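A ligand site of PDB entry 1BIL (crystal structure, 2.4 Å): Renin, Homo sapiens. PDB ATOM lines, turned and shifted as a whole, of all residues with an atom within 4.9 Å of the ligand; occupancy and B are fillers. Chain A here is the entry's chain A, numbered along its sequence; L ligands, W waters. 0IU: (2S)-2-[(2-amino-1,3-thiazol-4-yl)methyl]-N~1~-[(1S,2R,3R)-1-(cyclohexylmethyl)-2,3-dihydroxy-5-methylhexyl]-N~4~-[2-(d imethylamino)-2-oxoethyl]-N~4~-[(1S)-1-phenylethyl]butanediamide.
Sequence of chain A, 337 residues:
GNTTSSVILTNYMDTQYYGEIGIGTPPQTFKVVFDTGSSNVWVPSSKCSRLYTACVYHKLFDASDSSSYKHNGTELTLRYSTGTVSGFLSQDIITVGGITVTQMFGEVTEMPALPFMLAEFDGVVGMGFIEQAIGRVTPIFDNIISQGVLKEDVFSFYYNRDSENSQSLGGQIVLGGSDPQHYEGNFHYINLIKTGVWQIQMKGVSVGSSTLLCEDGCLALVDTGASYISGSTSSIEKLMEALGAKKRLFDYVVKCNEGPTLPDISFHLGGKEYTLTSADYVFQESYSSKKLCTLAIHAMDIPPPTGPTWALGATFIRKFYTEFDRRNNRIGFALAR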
ATOM      1  N   THR A  15      24.272  -4.573  -9.316  1.00  0.00           N
ATOM      2  CA  THR A  15      23.510  -3.493  -9.935  1.00  0.00           C
ATOM      3  C   THR A  15      22.660  -3.929 -11.104  1.00  0.00           C
ATOM      4  O   THR A  15      21.612  -3.335 -11.402  1.00  0.00           O
ATOM      5  CB  THR A  15      24.479  -2.423 -10.404  1.00  0.00           C
ATOM      6  OG1 THR A  15      25.469  -3.121 -11.128  1.00  0.00           O
ATOM      7  CG2 THR A  15      25.131  -1.733  -9.207  1.00  0.00           C
ATOM      8  N   GLN A  16      23.114  -4.974 -11.799  1.00  0.00           N
ATOM      9  CA  GLN A  16      22.326  -5.532 -12.892  1.00  0.00           C
ATOM     10  C   GLN A  16      22.019  -7.002 -12.633  1.00  0.00           C
ATOM     11  O   GLN A  16      22.915  -7.792 -12.435  1.00  0.00           O
ATOM     12  CB  GLN A  16      22.975  -5.353 -14.280  1.00  0.00           C
ATOM     13  CG  GLN A  16      23.744  -4.054 -14.427  1.00  0.00           C
ATOM     14  CD  GLN A  16      24.304  -3.904 -15.806  1.00  0.00           C
ATOM     15  OE1 GLN A  16      23.917  -4.623 -16.731  1.00  0.00           O
ATOM     16  NE2 GLN A  16      25.275  -3.030 -15.964  1.00  0.00           N
ATOM     17  N   VAL A  33      16.458  -7.858 -18.257  1.00  0.00           N
ATOM     18  CA  VAL A  33      16.190  -7.494 -16.928  1.00  0.00           C
ATOM     19  C   VAL A  33      14.683  -7.583 -16.800  1.00  0.00           C
ATOM     20  O   VAL A  33      13.915  -7.300 -17.757  1.00  0.00           O
ATOM     21  CB  VAL A  33      16.723  -6.086 -16.827  1.00  0.00           C
ATOM     22  CG1 VAL A  33      16.094  -5.393 -15.659  1.00  0.00           C
ATOM     23  CG2 VAL A  33      18.234  -6.109 -16.674  1.00  0.00           C
ATOM     24  N   ASP A  35      11.676  -6.069 -15.123  1.00  0.00           N
ATOM     25  CA  ASP A  35      11.339  -4.804 -14.505  1.00  0.00           C
ATOM     26  C   ASP A  35       9.875  -4.559 -14.216  1.00  0.00           C
ATOM     27  O   ASP A  35       9.097  -4.394 -15.152  1.00  0.00           O
ATOM     28  CB  ASP A  35      11.876  -3.695 -15.436  1.00  0.00           C
ATOM     29  CG  ASP A  35      11.337  -2.336 -15.166  1.00  0.00           C
ATOM     30  OD1 ASP A  35      11.414  -1.810 -14.083  1.00  0.00           O
ATOM     31  OD2 ASP A  35      10.891  -1.720 -16.223  1.00  0.00           O
ATOM     32  N   GLY A  37       8.677  -1.859 -12.858  1.00  0.00           N
ATOM     33  CA  GLY A  37       8.317  -0.466 -13.024  1.00  0.00           C
ATOM     34  C   GLY A  37       7.847  -0.174 -14.425  1.00  0.00           C
ATOM     35  O   GLY A  37       7.534   0.969 -14.710  1.00  0.00           O
ATOM     36  N   ARG A  79      10.207   5.354 -22.750  1.00  0.00           N
ATOM     37  CA  ARG A  79      10.908   6.254 -21.855  1.00  0.00           C
ATOM     38  C   ARG A  79      11.126   5.672 -20.463  1.00  0.00           C
ATOM     39  O   ARG A  79      10.224   5.152 -19.846  1.00  0.00           O
ATOM     40  CB  ARG A  79      10.203   7.586 -21.771  1.00  0.00           C
ATOM     41  CG  ARG A  79      10.164   8.355 -23.108  1.00  0.00           C
ATOM     42  CD  ARG A  79       9.483   9.699 -22.950  1.00  0.00           C
ATOM     43  NE  ARG A  79       9.497  10.559 -24.140  1.00  0.00           N
ATOM     44  CZ  ARG A  79       8.964  10.281 -25.362  1.00  0.00           C
ATOM     45  NH1 ARG A  79       8.298   9.168 -25.685  1.00  0.00           N
ATOM     46  NH2 ARG A  79       9.038  11.192 -26.323  1.00  0.00           N
ATOM     47  N   TYR A  80      12.353   5.704 -19.979  1.00  0.00           N
ATOM     48  CA  TYR A  80      12.620   5.190 -18.667  1.00  0.00           C
ATOM     49  C   TYR A  80      13.232   6.346 -17.963  1.00  0.00           C
ATOM     50  O   TYR A  80      13.601   7.304 -18.609  1.00  0.00           O
ATOM     51  CB  TYR A  80      13.628   4.018 -18.651  1.00  0.00           C
ATOM     52  CG  TYR A  80      13.078   2.799 -19.324  1.00  0.00           C
ATOM     53  CD1 TYR A  80      12.123   2.017 -18.669  1.00  0.00           C
ATOM     54  CD2 TYR A  80      13.435   2.479 -20.628  1.00  0.00           C
ATOM     55  CE1 TYR A  80      11.562   0.907 -19.296  1.00  0.00           C
ATOM     56  CE2 TYR A  80      12.855   1.389 -21.280  1.00  0.00           C
ATOM     57  CZ  TYR A  80      11.918   0.610 -20.608  1.00  0.00           C
ATOM     58  OH  TYR A  80      11.310  -0.448 -21.221  1.00  0.00           O
ATOM     59  N   SER A  81      13.365   6.218 -16.666  1.00  0.00           N
ATOM     60  CA  SER A  81      13.935   7.248 -15.888  1.00  0.00           C
ATOM     61  C   SER A  81      15.277   7.605 -16.421  1.00  0.00           C
ATOM     62  O   SER A  81      15.659   8.757 -16.376  1.00  0.00           O
ATOM     63  CB  SER A  81      14.106   6.760 -14.465  1.00  0.00           C
ATOM     64  OG  SER A  81      12.836   6.675 -13.878  1.00  0.00           O
ATOM     65  N   THR A  82      16.050   6.630 -16.865  1.00  0.00           N
ATOM     66  CA  THR A  82      17.415   6.924 -17.156  1.00  0.00           C
ATOM     67  C   THR A  82      17.814   6.835 -18.602  1.00  0.00           C
ATOM     68  O   THR A  82      19.021   6.735 -18.898  1.00  0.00           O
ATOM     69  CB  THR A  82      18.330   6.029 -16.299  1.00  0.00           C
ATOM     70  OG1 THR A  82      17.927   4.698 -16.496  1.00  0.00           O
ATOM     71  CG2 THR A  82      18.194   6.366 -14.826  1.00  0.00           C
ATOM     72  N   PRO A 115      22.192   4.926 -21.216  1.00  0.00           N
ATOM     73  CA  PRO A 115      22.977   4.042 -20.420  1.00  0.00           C
ATOM     74  C   PRO A 115      23.423   2.732 -21.052  1.00  0.00           C
ATOM     75  O   PRO A 115      24.240   2.040 -20.483  1.00  0.00           O
ATOM     76  CB  PRO A 115      22.050   3.738 -19.247  1.00  0.00           C
ATOM     77  CG  PRO A 115      20.651   3.744 -19.834  1.00  0.00           C
ATOM     78  CD  PRO A 115      20.727   4.756 -20.949  1.00  0.00           C
ATOM     79  N   PHE A 116      22.888   2.360 -22.195  1.00  0.00           N
ATOM     80  CA  PHE A 116      23.024   1.025 -22.750  1.00  0.00           C
ATOM     81  C   PHE A 116      24.378   0.377 -22.988  1.00  0.00           C
ATOM     82  O   PHE A 116      24.457  -0.851 -23.120  1.00  0.00           O
ATOM     83  CB  PHE A 116      22.032   0.788 -23.891  1.00  0.00           C
ATOM     84  CG  PHE A 116      20.629   1.076 -23.480  1.00  0.00           C
ATOM     85  CD1 PHE A 116      19.947   0.214 -22.632  1.00  0.00           C
ATOM     86  CD2 PHE A 116      20.039   2.310 -23.787  1.00  0.00           C
ATOM     87  CE1 PHE A 116      18.640   0.500 -22.222  1.00  0.00           C
ATOM     88  CE2 PHE A 116      18.760   2.631 -23.352  1.00  0.00           C
ATOM     89  CZ  PHE A 116      18.059   1.712 -22.572  1.00  0.00           C
ATOM     90  N   LEU A 118      26.632   0.517 -21.000  1.00  0.00           N
ATOM     91  CA  LEU A 118      27.067   0.041 -19.681  1.00  0.00           C
ATOM     92  C   LEU A 118      26.269  -1.182 -19.266  1.00  0.00           C
ATOM     93  O   LEU A 118      26.508  -1.789 -18.211  1.00  0.00           O
ATOM     94  CB  LEU A 118      26.886   1.161 -18.611  1.00  0.00           C
ATOM     95  CG  LEU A 118      27.489   2.488 -19.040  1.00  0.00           C
ATOM     96  CD1 LEU A 118      26.978   3.572 -18.135  1.00  0.00           C
ATOM     97  CD2 LEU A 118      28.991   2.409 -18.888  1.00  0.00           C
ATOM     98  N   ALA A 119      25.281  -1.552 -20.087  1.00  0.00           N
ATOM     99  CA  ALA A 119      24.417  -2.670 -19.772  1.00  0.00           C
ATOM    100  C   ALA A 119      25.004  -4.037 -20.103  1.00  0.00           C
ATOM    101  O   ALA A 119      25.347  -4.342 -21.250  1.00  0.00           O
ATOM    102  CB  ALA A 119      23.109  -2.536 -20.522  1.00  0.00           C
ATOM    103  N   PHE A 121      23.125  -6.605 -20.126  1.00  0.00           N
ATOM    104  CA  PHE A 121      21.970  -7.199 -20.780  1.00  0.00           C
ATOM    105  C   PHE A 121      21.658  -6.493 -22.088  1.00  0.00           C
ATOM    106  O   PHE A 121      22.314  -5.520 -22.438  1.00  0.00           O
ATOM    107  CB  PHE A 121      20.711  -7.207 -19.837  1.00  0.00           C
ATOM    108  CG  PHE A 121      20.437  -5.814 -19.286  1.00  0.00           C
ATOM    109  CD1 PHE A 121      21.179  -5.342 -18.210  1.00  0.00           C
ATOM    110  CD2 PHE A 121      19.522  -4.973 -19.896  1.00  0.00           C
ATOM    111  CE1 PHE A 121      20.962  -4.061 -17.710  1.00  0.00           C
ATOM    112  CE2 PHE A 121      19.311  -3.677 -19.435  1.00  0.00           C
ATOM    113  CZ  PHE A 121      20.049  -3.221 -18.352  1.00  0.00           C
ATOM    114  N   VAL A 124      14.699  -5.599 -21.967  1.00  0.00           N
ATOM    115  CA  VAL A 124      13.855  -5.580 -20.823  1.00  0.00           C
ATOM    116  C   VAL A 124      12.569  -6.333 -21.024  1.00  0.00           C
ATOM    117  O   VAL A 124      12.025  -6.345 -22.114  1.00  0.00           O
ATOM    118  CB  VAL A 124      13.536  -4.138 -20.470  1.00  0.00           C
ATOM    119  CG1 VAL A 124      12.732  -4.075 -19.158  1.00  0.00           C
ATOM    120  CG2 VAL A 124      14.858  -3.418 -20.231  1.00  0.00           C
ATOM    121  N   LEU A 221       7.228   2.766  -4.796  1.00  0.00           N
ATOM    122  CA  LEU A 221       7.083   1.872  -5.925  1.00  0.00           C
ATOM    123  C   LEU A 221       8.035   0.756  -5.643  1.00  0.00           C
ATOM    124  O   LEU A 221       9.168   1.061  -5.243  1.00  0.00           O
ATOM    125  CB  LEU A 221       7.661   2.601  -7.124  1.00  0.00           C
ATOM    126  CG  LEU A 221       7.418   2.002  -8.494  1.00  0.00           C
ATOM    127  CD1 LEU A 221       6.042   2.511  -8.964  1.00  0.00           C
ATOM    128  CD2 LEU A 221       8.479   2.628  -9.416  1.00  0.00           C
ATOM    129  N   ASP A 223      10.235  -1.626  -7.363  1.00  0.00           N
ATOM    130  CA  ASP A 223      10.698  -1.749  -8.741  1.00  0.00           C
ATOM    131  C   ASP A 223      12.009  -2.483  -8.879  1.00  0.00           C
ATOM    132  O   ASP A 223      13.071  -2.011  -8.528  1.00  0.00           O
ATOM    133  CB  ASP A 223      10.768  -0.293  -9.290  1.00  0.00           C
ATOM    134  CG  ASP A 223      11.473  -0.113 -10.564  1.00  0.00           C
ATOM    135  OD1 ASP A 223      11.767  -1.017 -11.267  1.00  0.00           O
ATOM    136  OD2 ASP A 223      11.831   1.109 -10.802  1.00  0.00           O
ATOM    137  N   GLY A 225      13.512  -3.212 -11.502  1.00  0.00           N
ATOM    138  CA  GLY A 225      14.297  -2.683 -12.601  1.00  0.00           C
ATOM    139  C   GLY A 225      15.176  -1.470 -12.238  1.00  0.00           C
ATOM    140  O   GLY A 225      15.601  -0.714 -13.110  1.00  0.00           O
ATOM    141  N   ALA A 226      15.402  -1.290 -10.938  1.00  0.00           N
ATOM    142  CA  ALA A 226      16.179  -0.198 -10.371  1.00  0.00           C
ATOM    143  C   ALA A 226      17.285  -0.717  -9.427  1.00  0.00           C
ATOM    144  O   ALA A 226      17.047  -1.399  -8.441  1.00  0.00           O
ATOM    145  CB  ALA A 226      15.233   0.774  -9.622  1.00  0.00           C
ATOM    146  N   SER A 227      18.547  -0.424  -9.698  1.00  0.00           N
ATOM    147  CA  SER A 227      19.605  -0.923  -8.830  1.00  0.00           C
ATOM    148  C   SER A 227      19.556  -0.426  -7.410  1.00  0.00           C
ATOM    149  O   SER A 227      19.819  -1.163  -6.484  1.00  0.00           O
ATOM    150  CB  SER A 227      20.983  -0.552  -9.349  1.00  0.00           C
ATOM    151  OG  SER A 227      21.045  -0.501 -10.765  1.00  0.00           O
ATOM    152  N   TYR A 228      19.261   0.857  -7.254  1.00  0.00           N
ATOM    153  CA  TYR A 228      19.241   1.562  -5.994  1.00  0.00           C
ATOM    154  C   TYR A 228      17.860   1.964  -5.473  1.00  0.00           C
ATOM    155  O   TYR A 228      16.859   1.824  -6.125  1.00  0.00           O
ATOM    156  CB  TYR A 228      20.005   2.853  -6.208  1.00  0.00           C
ATOM    157  CG  TYR A 228      21.485   2.727  -6.410  1.00  0.00           C
ATOM    158  CD1 TYR A 228      22.145   1.512  -6.629  1.00  0.00           C
ATOM    159  CD2 TYR A 228      22.220   3.899  -6.439  1.00  0.00           C
ATOM    160  CE1 TYR A 228      23.530   1.474  -6.742  1.00  0.00           C
ATOM    161  CE2 TYR A 228      23.597   3.884  -6.635  1.00  0.00           C
ATOM    162  CZ  TYR A 228      24.248   2.665  -6.827  1.00  0.00           C
ATOM    163  OH  TYR A 228      25.619   2.663  -6.970  1.00  0.00           O
ATOM    164  N   ILE A 229      17.831   2.386  -4.239  1.00  0.00           N
ATOM    165  CA  ILE A 229      16.614   2.880  -3.641  1.00  0.00           C
ATOM    166  C   ILE A 229      16.610   4.331  -4.045  1.00  0.00           C
ATOM    167  O   ILE A 229      17.704   4.861  -4.174  1.00  0.00           O
ATOM    168  CB  ILE A 229      16.554   2.792  -2.103  1.00  0.00           C
ATOM    169  CG1 ILE A 229      16.586   1.333  -1.596  1.00  0.00           C
ATOM    170  CG2 ILE A 229      15.331   3.527  -1.554  1.00  0.00           C
ATOM    171  CD1 ILE A 229      16.553   1.214  -0.064  1.00  0.00           C
ATOM    172  N   SER A 230      15.440   4.939  -4.274  1.00  0.00           N
ATOM    173  CA  SER A 230      15.369   6.315  -4.668  1.00  0.00           C
ATOM    174  C   SER A 230      14.264   7.100  -3.989  1.00  0.00           C
ATOM    175  O   SER A 230      13.208   6.652  -3.665  1.00  0.00           O
ATOM    176  CB  SER A 230      15.342   6.492  -6.168  1.00  0.00           C
ATOM    177  OG  SER A 230      14.063   6.170  -6.661  1.00  0.00           O
ATOM    178  N   HIS A 298      19.753   6.958  -4.127  1.00  0.00           N
ATOM    179  CA  HIS A 298      19.918   8.181  -4.872  1.00  0.00           C
ATOM    180  C   HIS A 298      18.605   8.839  -5.171  1.00  0.00           C
ATOM    181  O   HIS A 298      17.542   8.381  -4.755  1.00  0.00           O
ATOM    182  CB  HIS A 298      20.833   8.046  -6.096  1.00  0.00           C
ATOM    183  CG  HIS A 298      20.209   7.190  -7.150  1.00  0.00           C
ATOM    184  ND1 HIS A 298      20.893   6.840  -8.290  1.00  0.00           N
ATOM    185  CD2 HIS A 298      19.022   6.576  -7.181  1.00  0.00           C
ATOM    186  CE1 HIS A 298      20.097   6.047  -9.008  1.00  0.00           C
ATOM    187  NE2 HIS A 298      18.955   5.874  -8.372  1.00  0.00           N
ATOM    188  N   MET A 300      15.651  10.487  -7.501  1.00  0.00           N
ATOM    189  CA  MET A 300      15.035  10.306  -8.768  1.00  0.00           C
ATOM    190  C   MET A 300      13.702  10.955  -8.703  1.00  0.00           C
ATOM    191  O   MET A 300      12.890  10.621  -7.858  1.00  0.00           O
ATOM    192  CB  MET A 300      14.986   8.859  -9.166  1.00  0.00           C
ATOM    193  CG  MET A 300      14.745   8.715 -10.646  1.00  0.00           C
ATOM    194  SD  MET A 300      16.257   8.792 -11.677  1.00  0.00           S
ATOM    195  CE  MET A 300      17.374   7.547 -10.989  1.00  0.00           C
ATOM    196  N   ILE A 302      10.356  11.274 -10.132  1.00  0.00           N
ATOM    197  CA  ILE A 302       9.382  10.574 -10.978  1.00  0.00           C
ATOM    198  C   ILE A 302       8.153  11.432 -11.273  1.00  0.00           C
ATOM    199  O   ILE A 302       7.510  11.917 -10.375  1.00  0.00           O
ATOM    200  CB  ILE A 302       9.027   9.223 -10.366  1.00  0.00           C
ATOM    201  CG1 ILE A 302      10.325   8.400 -10.257  1.00  0.00           C
ATOM    202  CG2 ILE A 302       8.016   8.505 -11.248  1.00  0.00           C
ATOM    203  CD1 ILE A 302      10.189   7.188  -9.352  1.00  0.00           C
ATOM    204  N   THR A 306       2.735   8.321 -11.763  1.00  0.00           N
ATOM    205  CA  THR A 306       3.334   7.504 -10.752  1.00  0.00           C
ATOM    206  C   THR A 306       3.914   8.322  -9.622  1.00  0.00           C
ATOM    207  O   THR A 306       3.648   8.075  -8.429  1.00  0.00           O
ATOM    208  CB  THR A 306       4.442   6.595 -11.311  1.00  0.00           C
ATOM    209  OG1 THR A 306       3.892   5.715 -12.250  1.00  0.00           O
ATOM    210  CG2 THR A 306       5.143   5.812 -10.198  1.00  0.00           C
ATOM    211  N   ALA A 311      11.288   4.707  -4.668  1.00  0.00           N
ATOM    212  CA  ALA A 311      11.287   3.464  -5.443  1.00  0.00           C
ATOM    213  C   ALA A 311      12.168   2.485  -4.695  1.00  0.00           C
ATOM    214  O   ALA A 311      13.328   2.791  -4.361  1.00  0.00           O
ATOM    215  CB  ALA A 311      11.834   3.701  -6.856  1.00  0.00           C
HETATM  216  C1  0IU L   1      23.797   1.613 -11.242  1.00  0.00           C
HETATM  217  C2  0IU L   1      23.118   3.701 -10.002  1.00  0.00           C
HETATM  218  C   0IU L   1      21.702   2.782 -11.746  1.00  0.00           C
HETATM  219  O   0IU L   1      20.892   3.633 -11.545  1.00  0.00           O
HETATM  220  N   0IU L   1      22.845   2.722 -11.027  1.00  0.00           N
HETATM  221  N1  0IU L   1      20.306   2.150 -13.672  1.00  0.00           N
HETATM  222  C3  0IU L   1      19.105   2.011 -13.145  1.00  0.00           C
HETATM  223  O1  0IU L   1      19.059   1.676 -11.991  1.00  0.00           O
HETATM  224  CA  0IU L   1      21.468   1.787 -12.856  1.00  0.00           C
HETATM  225  CB  0IU L   1      20.473   2.686 -15.001  1.00  0.00           C
HETATM  226  CG2 0IU L   1      21.399   3.930 -14.830  1.00  0.00           C
HETATM  227  CG  0IU L   1      21.235   1.644 -15.851  1.00  0.00           C
HETATM  228  CD1 0IU L   1      22.301   1.994 -16.537  1.00  0.00           C
HETATM  229  CD2 0IU L   1      20.864   0.393 -15.834  1.00  0.00           C
HETATM  230  CE1 0IU L   1      23.014   1.067 -17.205  1.00  0.00           C
HETATM  231  CE2 0IU L   1      21.544  -0.521 -16.510  1.00  0.00           C
HETATM  232  CZ  0IU L   1      22.614  -0.183 -17.218  1.00  0.00           C
HETATM  233  C4  0IU L   1      15.541   2.752 -14.038  1.00  0.00           C
HETATM  234  O2  0IU L   1      15.502   3.719 -14.815  1.00  0.00           O
HETATM  235  CA1 0IU L   1      16.664   2.700 -13.048  1.00  0.00           C
HETATM  236  CN  0IU L   1      17.865   2.330 -13.951  1.00  0.00           C
HETATM  237  CB1 0IU L   1      16.903   4.104 -12.458  1.00  0.00           C
HETATM  238  CG1 0IU L   1      15.993   4.278 -11.258  1.00  0.00           C
HETATM  239 CD21 0IU L   1      14.816   4.837 -11.412  1.00  0.00           C
HETATM  240  SE2 0IU L   1      13.903   4.786  -9.898  1.00  0.00           S
HETATM  241 CE11 0IU L   1      15.310   4.004  -9.227  1.00  0.00           C
HETATM  242  ND1 0IU L   1      16.260   3.819 -10.043  1.00  0.00           N
HETATM  243  NZ  0IU L   1      15.318   3.694  -7.966  1.00  0.00           N
HETATM  244  C11 0IU L   1      12.294   1.532 -14.728  1.00  0.00           C
HETATM  245  C21 0IU L   1      13.747   1.571 -15.253  1.00  0.00           C
HETATM  246  C31 0IU L   1      14.001   0.319 -16.161  1.00  0.00           C
HETATM  247  C1' 0IU L   1      15.498   0.036 -16.456  1.00  0.00           C
HETATM  248  C2' 0IU L   1      15.686  -1.444 -16.964  1.00  0.00           C
HETATM  249  C3' 0IU L   1      17.158  -1.648 -17.435  1.00  0.00           C
HETATM  250  C4' 0IU L   1      17.457  -0.689 -18.625  1.00  0.00           C
HETATM  251  C5' 0IU L   1      17.382   0.743 -18.046  1.00  0.00           C
HETATM  252  C6' 0IU L   1      15.904   0.966 -17.594  1.00  0.00           C
HETATM  253  N2  0IU L   1      14.750   1.648 -14.187  1.00  0.00           N
HETATM  254  O11 0IU L   1      12.194   0.746 -13.534  1.00  0.00           O
HETATM  255  C12 0IU L   1      11.796   2.951 -14.415  1.00  0.00           C
HETATM  256  C22 0IU L   1      10.346   2.854 -13.855  1.00  0.00           C
HETATM  257  C32 0IU L   1       9.864   4.259 -13.401  1.00  0.00           C
HETATM  258  C41 0IU L   1       8.346   4.359 -13.310  1.00  0.00           C
HETATM  259  C5  0IU L   1      10.502   4.578 -12.032  1.00  0.00           C
HETATM  260  O12 0IU L   1      11.788   3.640 -15.649  1.00  0.00           O
HETATM  261  O   HOH W   1       9.625   4.367 -17.219  1.00  0.00           O
HETATM  262  O   HOH W   2      18.726   3.241  -9.361  1.00  0.00           O
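Merely in contact with the ligand: Pro 115, Ala 226, Phe 121, Tyr 80, Gly 37, Met 300, His 298, Ala 311, Ile 302, Leu 221, Val 124, Phe 116 and Ala 119. Hydrophobic or aromatic side chains within 4 Å of the ligand: Tyr 80, Pro 115, Phe 116, Phe 121, Val 124, Leu 221, Ala 226, Tyr 228, His 298, Met 300, Ile 302 and Ala 311. 21 residues have an atom within 4 Å of the ligand: Asp 35, Gly 37, Tyr 80, Ser 81, Thr 82, Pro 115, Phe 116, Ala 119, Phe 121, Val 124, Leu 221, Asp 223, Gly 225, Ala 226, Ser 227, Tyr 228, Ser 230, His 298, Met 300, Ile 302 and Ala 311.
Water W2 lies within hydrogen-bond range of ND1 of the ligand (2.6 Å), NE2 of His 298 (2.8 Å) and N of Tyr 228 (3.2 Å). Water W1 lies within hydrogen-bond range of O12 of the ligand (2.8 Å) and O of Arg 79 (2.8 Å).
OD1 of Asp 35 lies within hydrogen-bond range of N of Gly 37 (3.0 Å). OD1 of Asp 223 is in hydrogen-bond range of N of Gly 225 (2.8 Å). The backbone carbonyl oxygen (O) of Ser 230 lies within hydrogen-bond range of the backbone NH (N) of Ala 311, 2.9 Å away. The side-chain hydroxyl (OG) of Ser 227 is in hydrogen-bond range of the backbone carbonyl oxygen (O) of Thr 15, 3.0 Å away. The backbone carbonyl oxygen (O) of Ile 229 lies within hydrogen-bond range of the backbone NH (N) of His 298, at 2.9 Å.
The side-chain carboxylate of Asp 35 lies within hydrogen-bond range of an oxygen (O11) of the ligand (2.7 Å). The backbone carbonyl oxygen (O) of Gly 225 sits at hydrogen-bond distance from a nitrogen (N2) of the ligand (2.7 Å). The side-chain carboxylate (OD2) of Asp 223 lies within hydrogen-bond range of an oxygen (O11) of the ligand. The backbone carbonyl oxygen (O) of Tyr 228 lies within hydrogen-bond range of a nitrogen (NZ) of the ligand, 3.0 Å away. OG of Ser 230 lies within hydrogen-bond range of NZ of the ligand (3.1 Å). The side-chain hydroxyl of Thr 82 lies within hydrogen-bond range of an oxygen (O2) of the ligand. The backbone NH (N) of Ser 227 sits at hydrogen-bond distance from an oxygen (O1) of the ligand (3.2 Å). OG of Ser 227 sits close to O1 of the ligand (3.2 Å). N of Ser 81 lies within hydrogen-bond range of O12 of the ligand (3.2 Å).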
